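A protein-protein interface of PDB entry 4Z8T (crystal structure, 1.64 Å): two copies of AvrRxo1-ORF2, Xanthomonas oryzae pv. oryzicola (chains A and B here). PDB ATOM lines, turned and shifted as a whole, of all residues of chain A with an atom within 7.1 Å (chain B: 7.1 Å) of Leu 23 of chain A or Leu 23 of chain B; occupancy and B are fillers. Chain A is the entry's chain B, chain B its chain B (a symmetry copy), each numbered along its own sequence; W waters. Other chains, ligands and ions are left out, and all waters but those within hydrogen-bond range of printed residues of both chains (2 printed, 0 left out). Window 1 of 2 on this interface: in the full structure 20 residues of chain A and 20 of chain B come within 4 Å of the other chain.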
ATOM      1  N   LEU A  16     -14.447  -6.599  -8.152  1.00  0.00           N
ATOM      2  CA  LEU A  16     -13.009  -6.551  -7.947  1.00  0.00           C
ATOM      3  C   LEU A  16     -12.534  -7.702  -7.052  1.00  0.00           C
ATOM      4  O   LEU A  16     -11.471  -8.271  -7.284  1.00  0.00           O
ATOM      5  CB  LEU A  16     -12.584  -5.189  -7.367  1.00  0.00           C
ATOM      6  CG  LEU A  16     -11.093  -4.970  -7.152  1.00  0.00           C
ATOM      7  CD1 LEU A  16     -10.264  -5.190  -8.435  1.00  0.00           C
ATOM      8  CD2 LEU A  16     -10.905  -3.552  -6.635  1.00  0.00           C
ATOM      9  N   LYS A  17     -13.316  -8.048  -6.031  1.00  0.00           N
ATOM     10  CA  LYS A  17     -13.010  -9.218  -5.212  1.00  0.00           C
ATOM     11  C   LYS A  17     -12.966 -10.490  -6.059  1.00  0.00           C
ATOM     12  O   LYS A  17     -12.087 -11.332  -5.875  1.00  0.00           O
ATOM     13  CB  LYS A  17     -14.044  -9.392  -4.106  1.00  0.00           C
ATOM     14  CG  LYS A  17     -13.776  -8.573  -2.865  1.00  0.00           C
ATOM     15  CD  LYS A  17     -14.860  -8.803  -1.812  1.00  0.00           C
ATOM     16  CE  LYS A  17     -14.854 -10.240  -1.330  1.00  0.00           C
ATOM     17  NZ  LYS A  17     -15.850 -10.463  -0.237  1.00  0.00           N
ATOM     18  N   GLU A  18     -13.919 -10.633  -6.973  1.00  0.00           N
ATOM     19  CA  GLU A  18     -13.920 -11.800  -7.859  1.00  0.00           C
ATOM     20  C   GLU A  18     -12.684 -11.848  -8.736  1.00  0.00           C
ATOM     21  O   GLU A  18     -12.072 -12.901  -8.901  1.00  0.00           O
ATOM     22  CB  GLU A  18     -15.170 -11.815  -8.738  1.00  0.00           C
ATOM     23  CG  GLU A  18     -16.451 -11.937  -7.966  1.00  0.00           C
ATOM     24  CD  GLU A  18     -17.667 -12.000  -8.874  1.00  0.00           C
ATOM     25  OE1 GLU A  18     -17.490 -12.009 -10.115  1.00  0.00           O
ATOM     26  OE2 GLU A  18     -18.799 -12.039  -8.343  1.00  0.00           O
ATOM     27  N   ARG A  19     -12.336 -10.704  -9.317  1.00  0.00           N
ATOM     28  CA  ARG A  19     -11.153 -10.592 -10.157  1.00  0.00           C
ATOM     29  C   ARG A  19      -9.912 -10.999  -9.385  1.00  0.00           C
ATOM     30  O   ARG A  19      -9.113 -11.805  -9.857  1.00  0.00           O
ATOM     31  CB  ARG A  19     -10.995  -9.150 -10.646  1.00  0.00           C
ATOM     32  CG  ARG A  19      -9.753  -8.892 -11.507  1.00  0.00           C
ATOM     33  CD  ARG A  19      -9.520  -7.393 -11.652  1.00  0.00           C
ATOM     34  NE  ARG A  19      -8.432  -7.064 -12.570  1.00  0.00           N
ATOM     35  CZ  ARG A  19      -8.575  -6.936 -13.888  1.00  0.00           C
ATOM     36  NH1 ARG A  19      -9.760  -7.103 -14.455  1.00  0.00           N
ATOM     37  NH2 ARG A  19      -7.533  -6.634 -14.643  1.00  0.00           N
ATOM     38  N   ASN A  20      -9.740 -10.434  -8.191  1.00  0.00           N
ATOM     39  CA  ASN A  20      -8.516 -10.682  -7.439  1.00  0.00           C
ATOM     40  C   ASN A  20      -8.447 -12.112  -6.917  1.00  0.00           C
ATOM     41  O   ASN A  20      -7.372 -12.677  -6.775  1.00  0.00           O
ATOM     42  CB  ASN A  20      -8.375  -9.669  -6.288  1.00  0.00           C
ATOM     43  CG  ASN A  20      -8.057  -8.273  -6.782  1.00  0.00           C
ATOM     44  OD1 ASN A  20      -7.609  -8.082  -7.925  1.00  0.00           O
ATOM     45  ND2 ASN A  20      -8.278  -7.280  -5.919  1.00  0.00           N
ATOM     46  N   LYS A  21      -9.607 -12.704  -6.659  1.00  0.00           N
ATOM     47  CA  LYS A  21      -9.666 -14.100  -6.242  1.00  0.00           C
ATOM     48  C   LYS A  21      -9.208 -15.011  -7.379  1.00  0.00           C
ATOM     49  O   LYS A  21      -8.466 -15.979  -7.163  1.00  0.00           O
ATOM     50  CB  LYS A  21     -11.094 -14.469  -5.840  1.00  0.00           C
ATOM     51  CG  LYS A  21     -11.259 -15.940  -5.489  1.00  0.00           C
ATOM     52  CD  LYS A  21     -12.708 -16.286  -5.146  1.00  0.00           C
ATOM     53  CE  LYS A  21     -12.779 -17.579  -4.329  1.00  0.00           C
ATOM     54  NZ  LYS A  21     -14.177 -18.053  -4.090  1.00  0.00           N
ATOM     55  N   ALA A  22      -9.651 -14.693  -8.590  1.00  0.00           N
ATOM     56  CA  ALA A  22      -9.251 -15.458  -9.767  1.00  0.00           C
ATOM     57  C   ALA A  22      -7.756 -15.319 -10.013  1.00  0.00           C
ATOM     58  O   ALA A  22      -7.087 -16.292 -10.364  1.00  0.00           O
ATOM     59  CB  ALA A  22     -10.043 -15.014 -10.992  1.00  0.00           C
ATOM     60  N   LEU A  23      -7.230 -14.112  -9.827  1.00  0.00           N
ATOM     61  CA  LEU A  23      -5.805 -13.859 -10.010  1.00  0.00           C
ATOM     62  C   LEU A  23      -4.993 -14.583  -8.940  1.00  0.00           C
ATOM     63  O   LEU A  23      -3.926 -15.129  -9.214  1.00  0.00           O
ATOM     64  CB  LEU A  23      -5.507 -12.358  -9.965  1.00  0.00           C
ATOM     65  CG  LEU A  23      -5.938 -11.505 -11.158  1.00  0.00           C
ATOM     66  CD1 LEU A  23      -5.781 -10.021 -10.843  1.00  0.00           C
ATOM     67  CD2 LEU A  23      -5.070 -11.869 -12.349  1.00  0.00           C
ATOM     68  N   HIS A  24      -5.516 -14.576  -7.721  1.00  0.00           N
ATOM     69  CA  HIS A  24      -4.873 -15.214  -6.581  1.00  0.00           C
ATOM     70  C   HIS A  24      -4.723 -16.714  -6.839  1.00  0.00           C
ATOM     71  O   HIS A  24      -3.648 -17.295  -6.650  1.00  0.00           O
ATOM     72  CB  HIS A  24      -5.746 -14.971  -5.353  1.00  0.00           C
ATOM     73  CG  HIS A  24      -5.074 -15.235  -4.046  1.00  0.00           C
ATOM     74  ND1 HIS A  24      -3.932 -14.576  -3.644  1.00  0.00           N
ATOM     75  CD2 HIS A  24      -5.411 -16.059  -3.023  1.00  0.00           C
ATOM     76  CE1 HIS A  24      -3.584 -14.996  -2.441  1.00  0.00           C
ATOM     77  NE2 HIS A  24      -4.463 -15.899  -2.043  1.00  0.00           N
ATOM     78  N   ALA A  25      -5.811 -17.347  -7.260  1.00  0.00           N
ATOM     79  CA  ALA A  25      -5.784 -18.776  -7.544  1.00  0.00           C
ATOM     80  C   ALA A  25      -4.895 -19.078  -8.746  1.00  0.00           C
ATOM     81  O   ALA A  25      -4.123 -20.040  -8.733  1.00  0.00           O
ATOM     82  CB  ALA A  25      -7.183 -19.291  -7.783  1.00  0.00           C
ATOM     83  N   SER A  26      -5.005 -18.250  -9.778  1.00  0.00           N
ATOM     84  CA  SER A  26      -4.211 -18.440 -10.985  1.00  0.00           C
ATOM     85  C   SER A  26      -2.701 -18.345 -10.757  1.00  0.00           C
ATOM     86  O   SER A  26      -1.936 -19.168 -11.285  1.00  0.00           O
ATOM     87  CB  SER A  26      -4.635 -17.444 -12.062  1.00  0.00           C
ATOM     88  OG  SER A  26      -3.792 -17.590 -13.181  1.00  0.00           O
ATOM     89  N   ASP A  27      -2.268 -17.347  -9.985  1.00  0.00           N
ATOM     90  CA  ASP A  27      -0.856 -17.208  -9.664  1.00  0.00           C
ATOM     91  C   ASP A  27      -0.295 -18.508  -9.096  1.00  0.00           C
ATOM     92  O   ASP A  27       0.819 -18.911  -9.444  1.00  0.00           O
ATOM     93  CB  ASP A  27      -0.618 -16.086  -8.640  1.00  0.00           C
ATOM     94  CG  ASP A  27      -0.775 -14.690  -9.226  1.00  0.00           C
ATOM     95  OD1 ASP A  27      -0.722 -14.529 -10.465  1.00  0.00           O
ATOM     96  OD2 ASP A  27      -0.940 -13.739  -8.426  1.00  0.00           O
ATOM     97  N   LEU A  28      -1.069 -19.158  -8.229  1.00  0.00           N
ATOM     98  CA  LEU A  28      -0.609 -20.387  -7.575  1.00  0.00           C
ATOM     99  C   LEU A  28      -0.652 -21.554  -8.547  1.00  0.00           C
ATOM    100  O   LEU A  28       0.304 -22.324  -8.628  1.00  0.00           O
ATOM    101  CB  LEU A  28      -1.427 -20.689  -6.316  1.00  0.00           C
ATOM    102  CG  LEU A  28      -1.069 -21.989  -5.580  1.00  0.00           C
ATOM    103  CD1 LEU A  28       0.395 -22.009  -5.197  1.00  0.00           C
ATOM    104  CD2 LEU A  28      -1.944 -22.171  -4.341  1.00  0.00           C
ATOM    105  N   GLU A  29      -1.733 -21.661  -9.312  1.00  0.00           N
ATOM    106  CA  GLU A  29      -1.852 -22.730 -10.310  1.00  0.00           C
ATOM    107  C   GLU A  29      -0.703 -22.687 -11.313  1.00  0.00           C
ATOM    108  O   GLU A  29      -0.061 -23.711 -11.576  1.00  0.00           O
ATOM    109  CB  GLU A  29      -3.178 -22.629 -11.055  1.00  0.00           C
ATOM    110  CG  GLU A  29      -4.399 -22.894 -10.207  1.00  0.00           C
ATOM    111  CD  GLU A  29      -5.661 -22.442 -10.898  1.00  0.00           C
ATOM    112  OE1 GLU A  29      -5.555 -21.759 -11.949  1.00  0.00           O
ATOM    113  OE2 GLU A  29      -6.758 -22.753 -10.391  1.00  0.00           O
ATOM    114  N   ARG A  72       1.904 -20.775  -0.526  1.00  0.00           N
ATOM    115  CA  ARG A  72       1.743 -19.754  -1.554  1.00  0.00           C
ATOM    116  C   ARG A  72       2.994 -18.888  -1.687  1.00  0.00           C
ATOM    117  O   ARG A  72       3.445 -18.608  -2.794  1.00  0.00           O
ATOM    118  CB  ARG A  72       0.512 -18.895  -1.266  1.00  0.00           C
ATOM    119  CG  ARG A  72       0.372 -17.707  -2.180  1.00  0.00           C
ATOM    120  CD  ARG A  72      -0.932 -16.971  -1.936  1.00  0.00           C
ATOM    121  NE  ARG A  72      -2.068 -17.786  -2.342  1.00  0.00           N
ATOM    122  CZ  ARG A  72      -2.453 -17.936  -3.608  1.00  0.00           C
ATOM    123  NH1 ARG A  72      -3.496 -18.699  -3.887  1.00  0.00           N
ATOM    124  NH2 ARG A  72      -1.793 -17.322  -4.594  1.00  0.00           N
ATOM    125  N   LEU B  16      -3.600 -20.718 -17.993  1.00  0.00           N
ATOM    126  CA  LEU B  16      -3.473 -19.358 -18.493  1.00  0.00           C
ATOM    127  C   LEU B  16      -4.738 -18.917 -19.239  1.00  0.00           C
ATOM    128  O   LEU B  16      -5.155 -17.768 -19.128  1.00  0.00           O
ATOM    129  CB  LEU B  16      -2.227 -19.218 -19.386  1.00  0.00           C
ATOM    130  CG  LEU B  16      -1.930 -17.830 -19.936  1.00  0.00           C
ATOM    131  CD1 LEU B  16      -1.813 -16.759 -18.831  1.00  0.00           C
ATOM    132  CD2 LEU B  16      -0.637 -17.915 -20.732  1.00  0.00           C
ATOM    133  N   LYS B  17      -5.350 -19.825 -19.999  1.00  0.00           N
ATOM    134  CA  LYS B  17      -6.631 -19.532 -20.634  1.00  0.00           C
ATOM    135  C   LYS B  17      -7.696 -19.178 -19.596  1.00  0.00           C
ATOM    136  O   LYS B  17      -8.480 -18.251 -19.797  1.00  0.00           O
ATOM    137  CB  LYS B  17      -7.114 -20.722 -21.455  1.00  0.00           C
ATOM    138  CG  LYS B  17      -6.546 -20.789 -22.853  1.00  0.00           C
ATOM    139  CD  LYS B  17      -7.076 -22.010 -23.603  1.00  0.00           C
ATOM    140  CE  LYS B  17      -8.575 -21.916 -23.805  1.00  0.00           C
ATOM    141  NZ  LYS B  17      -9.100 -23.060 -24.613  1.00  0.00           N
ATOM    142  N   GLU B  18      -7.730 -19.922 -18.496  1.00  0.00           N
ATOM    143  CA  GLU B  18      -8.688 -19.617 -17.430  1.00  0.00           C
ATOM    144  C   GLU B  18      -8.451 -18.245 -16.829  1.00  0.00           C
ATOM    145  O   GLU B  18      -9.393 -17.488 -16.602  1.00  0.00           O
ATOM    146  CB  GLU B  18      -8.629 -20.674 -16.328  1.00  0.00           C
ATOM    147  CG  GLU B  18      -9.014 -22.050 -16.787  1.00  0.00           C
ATOM    148  CD  GLU B  18      -8.994 -23.062 -15.654  1.00  0.00           C
ATOM    149  OE1 GLU B  18      -8.735 -22.661 -14.495  1.00  0.00           O
ATOM    150  OE2 GLU B  18      -9.236 -24.258 -15.927  1.00  0.00           O
ATOM    151  N   ARG B  19      -7.187 -17.940 -16.551  1.00  0.00           N
ATOM    152  CA  ARG B  19      -6.807 -16.647 -16.005  1.00  0.00           C
ATOM    153  C   ARG B  19      -7.256 -15.527 -16.925  1.00  0.00           C
ATOM    154  O   ARG B  19      -7.878 -14.563 -16.486  1.00  0.00           O
ATOM    155  CB  ARG B  19      -5.288 -16.581 -15.830  1.00  0.00           C
ATOM    156  CG  ARG B  19      -4.755 -15.243 -15.303  1.00  0.00           C
ATOM    157  CD  ARG B  19      -3.244 -15.174 -15.485  1.00  0.00           C
ATOM    158  NE  ARG B  19      -2.644 -13.985 -14.884  1.00  0.00           N
ATOM    159  CZ  ARG B  19      -2.263 -13.899 -13.611  1.00  0.00           C
ATOM    160  NH1 ARG B  19      -2.410 -14.930 -12.794  1.00  0.00           N
ATOM    161  NH2 ARG B  19      -1.727 -12.781 -13.152  1.00  0.00           N
ATOM    162  N   ASN B  20      -6.934 -15.648 -18.213  1.00  0.00           N
ATOM    163  CA  ASN B  20      -7.225 -14.561 -19.139  1.00  0.00           C
ATOM    164  C   ASN B  20      -8.720 -14.413 -19.394  1.00  0.00           C
ATOM    165  O   ASN B  20      -9.209 -13.321 -19.646  1.00  0.00           O
ATOM    166  CB  ASN B  20      -6.460 -14.759 -20.461  1.00  0.00           C
ATOM    167  CG  ASN B  20      -4.970 -14.530 -20.306  1.00  0.00           C
ATOM    168  OD1 ASN B  20      -4.513 -13.907 -19.333  1.00  0.00           O
ATOM    169  ND2 ASN B  20      -4.196 -15.026 -21.273  1.00  0.00           N
ATOM    170  N   LYS B  21      -9.448 -15.519 -19.297  1.00  0.00           N
ATOM    171  CA  LYS B  21     -10.900 -15.482 -19.431  1.00  0.00           C
ATOM    172  C   LYS B  21     -11.518 -14.715 -18.263  1.00  0.00           C
ATOM    173  O   LYS B  21     -12.443 -13.911 -18.445  1.00  0.00           O
ATOM    174  CB  LYS B  21     -11.462 -16.902 -19.459  1.00  0.00           C
ATOM    175  CG  LYS B  21     -12.982 -16.947 -19.493  1.00  0.00           C
ATOM    176  CD  LYS B  21     -13.513 -18.380 -19.465  1.00  0.00           C
ATOM    177  CE  LYS B  21     -14.947 -18.440 -19.999  1.00  0.00           C
ATOM    178  NZ  LYS B  21     -15.576 -19.789 -19.858  1.00  0.00           N
ATOM    179  N   ALA B  22     -10.999 -14.964 -17.067  1.00  0.00           N
ATOM    180  CA  ALA B  22     -11.471 -14.265 -15.876  1.00  0.00           C
ATOM    181  C   ALA B  22     -11.159 -12.778 -15.970  1.00  0.00           C
ATOM    182  O   ALA B  22     -11.980 -11.942 -15.590  1.00  0.00           O
ATOM    183  CB  ALA B  22     -10.856 -14.867 -14.618  1.00  0.00           C
ATOM    184  N   LEU B  23      -9.975 -12.448 -16.477  1.00  0.00           N
ATOM    185  CA  LEU B  23      -9.570 -11.056 -16.637  1.00  0.00           C
ATOM    186  C   LEU B  23     -10.425 -10.370 -17.699  1.00  0.00           C
ATOM    187  O   LEU B  23     -10.812  -9.212 -17.553  1.00  0.00           O
ATOM    188  CB  LEU B  23      -8.090 -10.958 -17.016  1.00  0.00           C
ATOM    189  CG  LEU B  23      -7.052 -11.264 -15.937  1.00  0.00           C
ATOM    190  CD1 LEU B  23      -5.655 -11.351 -16.544  1.00  0.00           C
ATOM    191  CD2 LEU B  23      -7.091 -10.154 -14.901  1.00  0.00           C
ATOM    192  N   HIS B  24     -10.711 -11.104 -18.766  1.00  0.00           N
ATOM    193  CA  HIS B  24     -11.511 -10.607 -19.876  1.00  0.00           C
ATOM    194  C   HIS B  24     -12.909 -10.229 -19.384  1.00  0.00           C
ATOM    195  O   HIS B  24     -13.423  -9.144 -19.679  1.00  0.00           O
ATOM    196  CB  HIS B  24     -11.599 -11.714 -20.925  1.00  0.00           C
ATOM    197  CG  HIS B  24     -12.065 -11.265 -22.270  1.00  0.00           C
ATOM    198  ND1 HIS B  24     -11.407 -10.306 -23.010  1.00  0.00           N
ATOM    199  CD2 HIS B  24     -13.105 -11.680 -23.034  1.00  0.00           C
ATOM    200  CE1 HIS B  24     -12.032 -10.135 -24.161  1.00  0.00           C
ATOM    201  NE2 HIS B  24     -13.068 -10.955 -24.199  1.00  0.00           N
ATOM    202  N   ALA B  25     -13.533 -11.135 -18.642  1.00  0.00           N
ATOM    203  CA  ALA B  25     -14.866 -10.881 -18.113  1.00  0.00           C
ATOM    204  C   ALA B  25     -14.840  -9.757 -17.082  1.00  0.00           C
ATOM    205  O   ALA B  25     -15.716  -8.888 -17.076  1.00  0.00           O
ATOM    206  CB  ALA B  25     -15.438 -12.138 -17.504  1.00  0.00           C
ATOM    207  N   SER B  26     -13.832  -9.777 -16.219  1.00  0.00           N
ATOM    208  CA  SER B  26     -13.704  -8.758 -15.185  1.00  0.00           C
ATOM    209  C   SER B  26     -13.530  -7.339 -15.729  1.00  0.00           C
ATOM    210  O   SER B  26     -14.161  -6.395 -15.226  1.00  0.00           O
ATOM    211  CB  SER B  26     -12.549  -9.097 -14.245  1.00  0.00           C
ATOM    212  OG  SER B  26     -12.393  -8.052 -13.314  1.00  0.00           O
ATOM    213  N   ASP B  27     -12.677  -7.181 -16.742  1.00  0.00           N
ATOM    214  CA  ASP B  27     -12.487  -5.879 -17.365  1.00  0.00           C
ATOM    215  C   ASP B  27     -13.824  -5.277 -17.786  1.00  0.00           C
ATOM    216  O   ASP B  27     -14.052  -4.076 -17.605  1.00  0.00           O
ATOM    217  CB  ASP B  27     -11.582  -5.973 -18.603  1.00  0.00           C
ATOM    218  CG  ASP B  27     -10.114  -6.191 -18.263  1.00  0.00           C
ATOM    219  OD1 ASP B  27      -9.700  -5.932 -17.112  1.00  0.00           O
ATOM    220  OD2 ASP B  27      -9.363  -6.615 -19.173  1.00  0.00           O
ATOM    221  N   LEU B  28     -14.700  -6.110 -18.344  1.00  0.00           N
ATOM    222  CA  LEU B  28     -15.992  -5.630 -18.841  1.00  0.00           C
ATOM    223  C   LEU B  28     -16.936  -5.350 -17.684  1.00  0.00           C
ATOM    224  O   LEU B  28     -17.590  -4.309 -17.661  1.00  0.00           O
ATOM    225  CB  LEU B  28     -16.613  -6.621 -19.831  1.00  0.00           C
ATOM    226  CG  LEU B  28     -18.000  -6.247 -20.373  1.00  0.00           C
ATOM    227  CD1 LEU B  28     -17.974  -4.887 -21.037  1.00  0.00           C
ATOM    228  CD2 LEU B  28     -18.504  -7.305 -21.354  1.00  0.00           C
ATOM    229  N   GLU B  29     -16.977  -6.252 -16.709  1.00  0.00           N
ATOM    230  CA  GLU B  29     -17.826  -6.054 -15.529  1.00  0.00           C
ATOM    231  C   GLU B  29     -17.483  -4.755 -14.807  1.00  0.00           C
ATOM    232  O   GLU B  29     -18.373  -3.954 -14.496  1.00  0.00           O
ATOM    233  CB  GLU B  29     -17.689  -7.223 -14.561  1.00  0.00           C
ATOM    234  CG  GLU B  29     -18.223  -8.537 -15.080  1.00  0.00           C
ATOM    235  CD  GLU B  29     -17.749  -9.697 -14.241  1.00  0.00           C
ATOM    236  OE1 GLU B  29     -16.859  -9.485 -13.377  1.00  0.00           O
ATOM    237  OE2 GLU B  29     -18.248 -10.821 -14.448  1.00  0.00           O
ATOM    238  N   ARG B  72     -17.594  -4.422 -26.062  1.00  0.00           N
ATOM    239  CA  ARG B  72     -16.402  -4.516 -25.227  1.00  0.00           C
ATOM    240  C   ARG B  72     -15.424  -3.378 -25.513  1.00  0.00           C
ATOM    241  O   ARG B  72     -14.888  -2.770 -24.591  1.00  0.00           O
ATOM    242  CB  ARG B  72     -15.727  -5.875 -25.411  1.00  0.00           C
ATOM    243  CG  ARG B  72     -14.394  -5.991 -24.721  1.00  0.00           C
ATOM    244  CD  ARG B  72     -13.837  -7.398 -24.825  1.00  0.00           C
ATOM    245  NE  ARG B  72     -14.645  -8.332 -24.054  1.00  0.00           N
ATOM    246  CZ  ARG B  72     -14.566  -8.456 -22.730  1.00  0.00           C
ATOM    247  NH1 ARG B  72     -15.342  -9.329 -22.110  1.00  0.00           N
ATOM    248  NH2 ARG B  72     -13.711  -7.707 -22.029  1.00  0.00           N
HETATM  249  O   HOH W   1      -6.909  -6.119 -17.072  1.00  0.00           O
HETATM  250  O   HOH W   2      -0.676 -11.791 -11.038  1.00  0.00           O
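OG of Ser 26 of chain B lies within hydrogen-bond range of NH1 of Arg 19 of chain A (3.0 Å). The guanidinium group (NH1) of Arg 19 of chain A is in salt-bridge range of the side-chain carboxylate (OD1) of Asp 27 of chain B, 2.9 Å away. The side-chain hydroxyl (OG) of Ser 26 of chain A sits at hydrogen-bond distance from the guanidinium group (NH1) of Arg 19 of chain B (3.0 Å). OD1 of Asp 27 of chain A is in salt-bridge range of NH1 of Arg 19 of chain B (2.9 Å).
CD2 of Leu 23 of chain B touches NH2 of Arg 19 of chain A, at 3.6 Å. Ala 22 of chain B touches Ala 22 of chain A. Leu 23 of chain A touches Arg 19 of chain B. Leu 23 of chain B touches Leu 23 of chain A.
Lys 17 of chain A touches none of the printed residues of chain B. Of the printed residues of chain B, Arg 19 of chain A touches Leu 23 (3.6 Å), Ser 26 (3.0 Å) and Asp 27 (2.9 Å). Leu 23 of chain A touches just these residues of chain B: Arg 19 and Leu 23. Of the printed residues of chain B, Asp 27 of chain A touches Arg 19 (2.9 Å). Of the printed residues of chain A, Arg 19 of chain B touches Leu 23, Ser 26 and Asp 27. Of chain A, only Arg 19 (3.6 Å) and Leu 23 (3.7 Å) come within 4 Å of Leu 23 of chain B. His 24 of chain B touches none of the printed residues of chain A. Of the printed residues of chain A, Ser 26 of chain B touches Arg 19 (3.0 Å). The nearest printed residue of chain B that does not touch Asp 27 of chain A is Leu 23 of chain B (8.4 Å).
Of the 15 printed residues of chain A, 5 touch a printed residue of chain B. Printed residues of chain A that touch a printed residue of chain B: Arg 19, Ala 22, Leu 23, Ser 26 and Asp 27. Hydrophobic or aromatic side chains of chain A that line the printed part of chain B: Ala 22 and Leu 23. Of the 15 printed residues of chain B, 5 touch a printed residue of chain A. Hydrophobic or aromatic side chains of chain B that line the printed part of chain A: Ala 22 and Leu 23. Among the printed residues, 8 pairs touch across the chains.
Arg 19 of chain A touches Leu 23 of chain B, and with the chains exchanged Leu 23 of chain A touches Arg 19 of chain B. Arg 19 of chain A touches Ser 26 of chain B, and with the chains exchanged Ser 26 of chain A touches Arg 19 of chain B. Arg 19 of chain A touches Asp 27 of chain B, and with the chains exchanged Asp 27 of chain A touches Arg 19 of chain B. Leu 23 of chain A touches its own counterpart, Leu 23 of chain B. 15 positions are printed for both chains. Of the 8 pairs that touch across the chains among the printed residues, 8 have their exchanged pair printed and touching as well.
Water W1 bridges NH2 of Arg 19 of chain A (2.6 Å) and OD1 of Asp 27 of chain B (2.8 Å). Water W2 bridges the guanidinium group of Arg 19 of chain B (2.6 Å) and the side-chain carboxylate of Asp 27 of chain A (2.8 Å).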
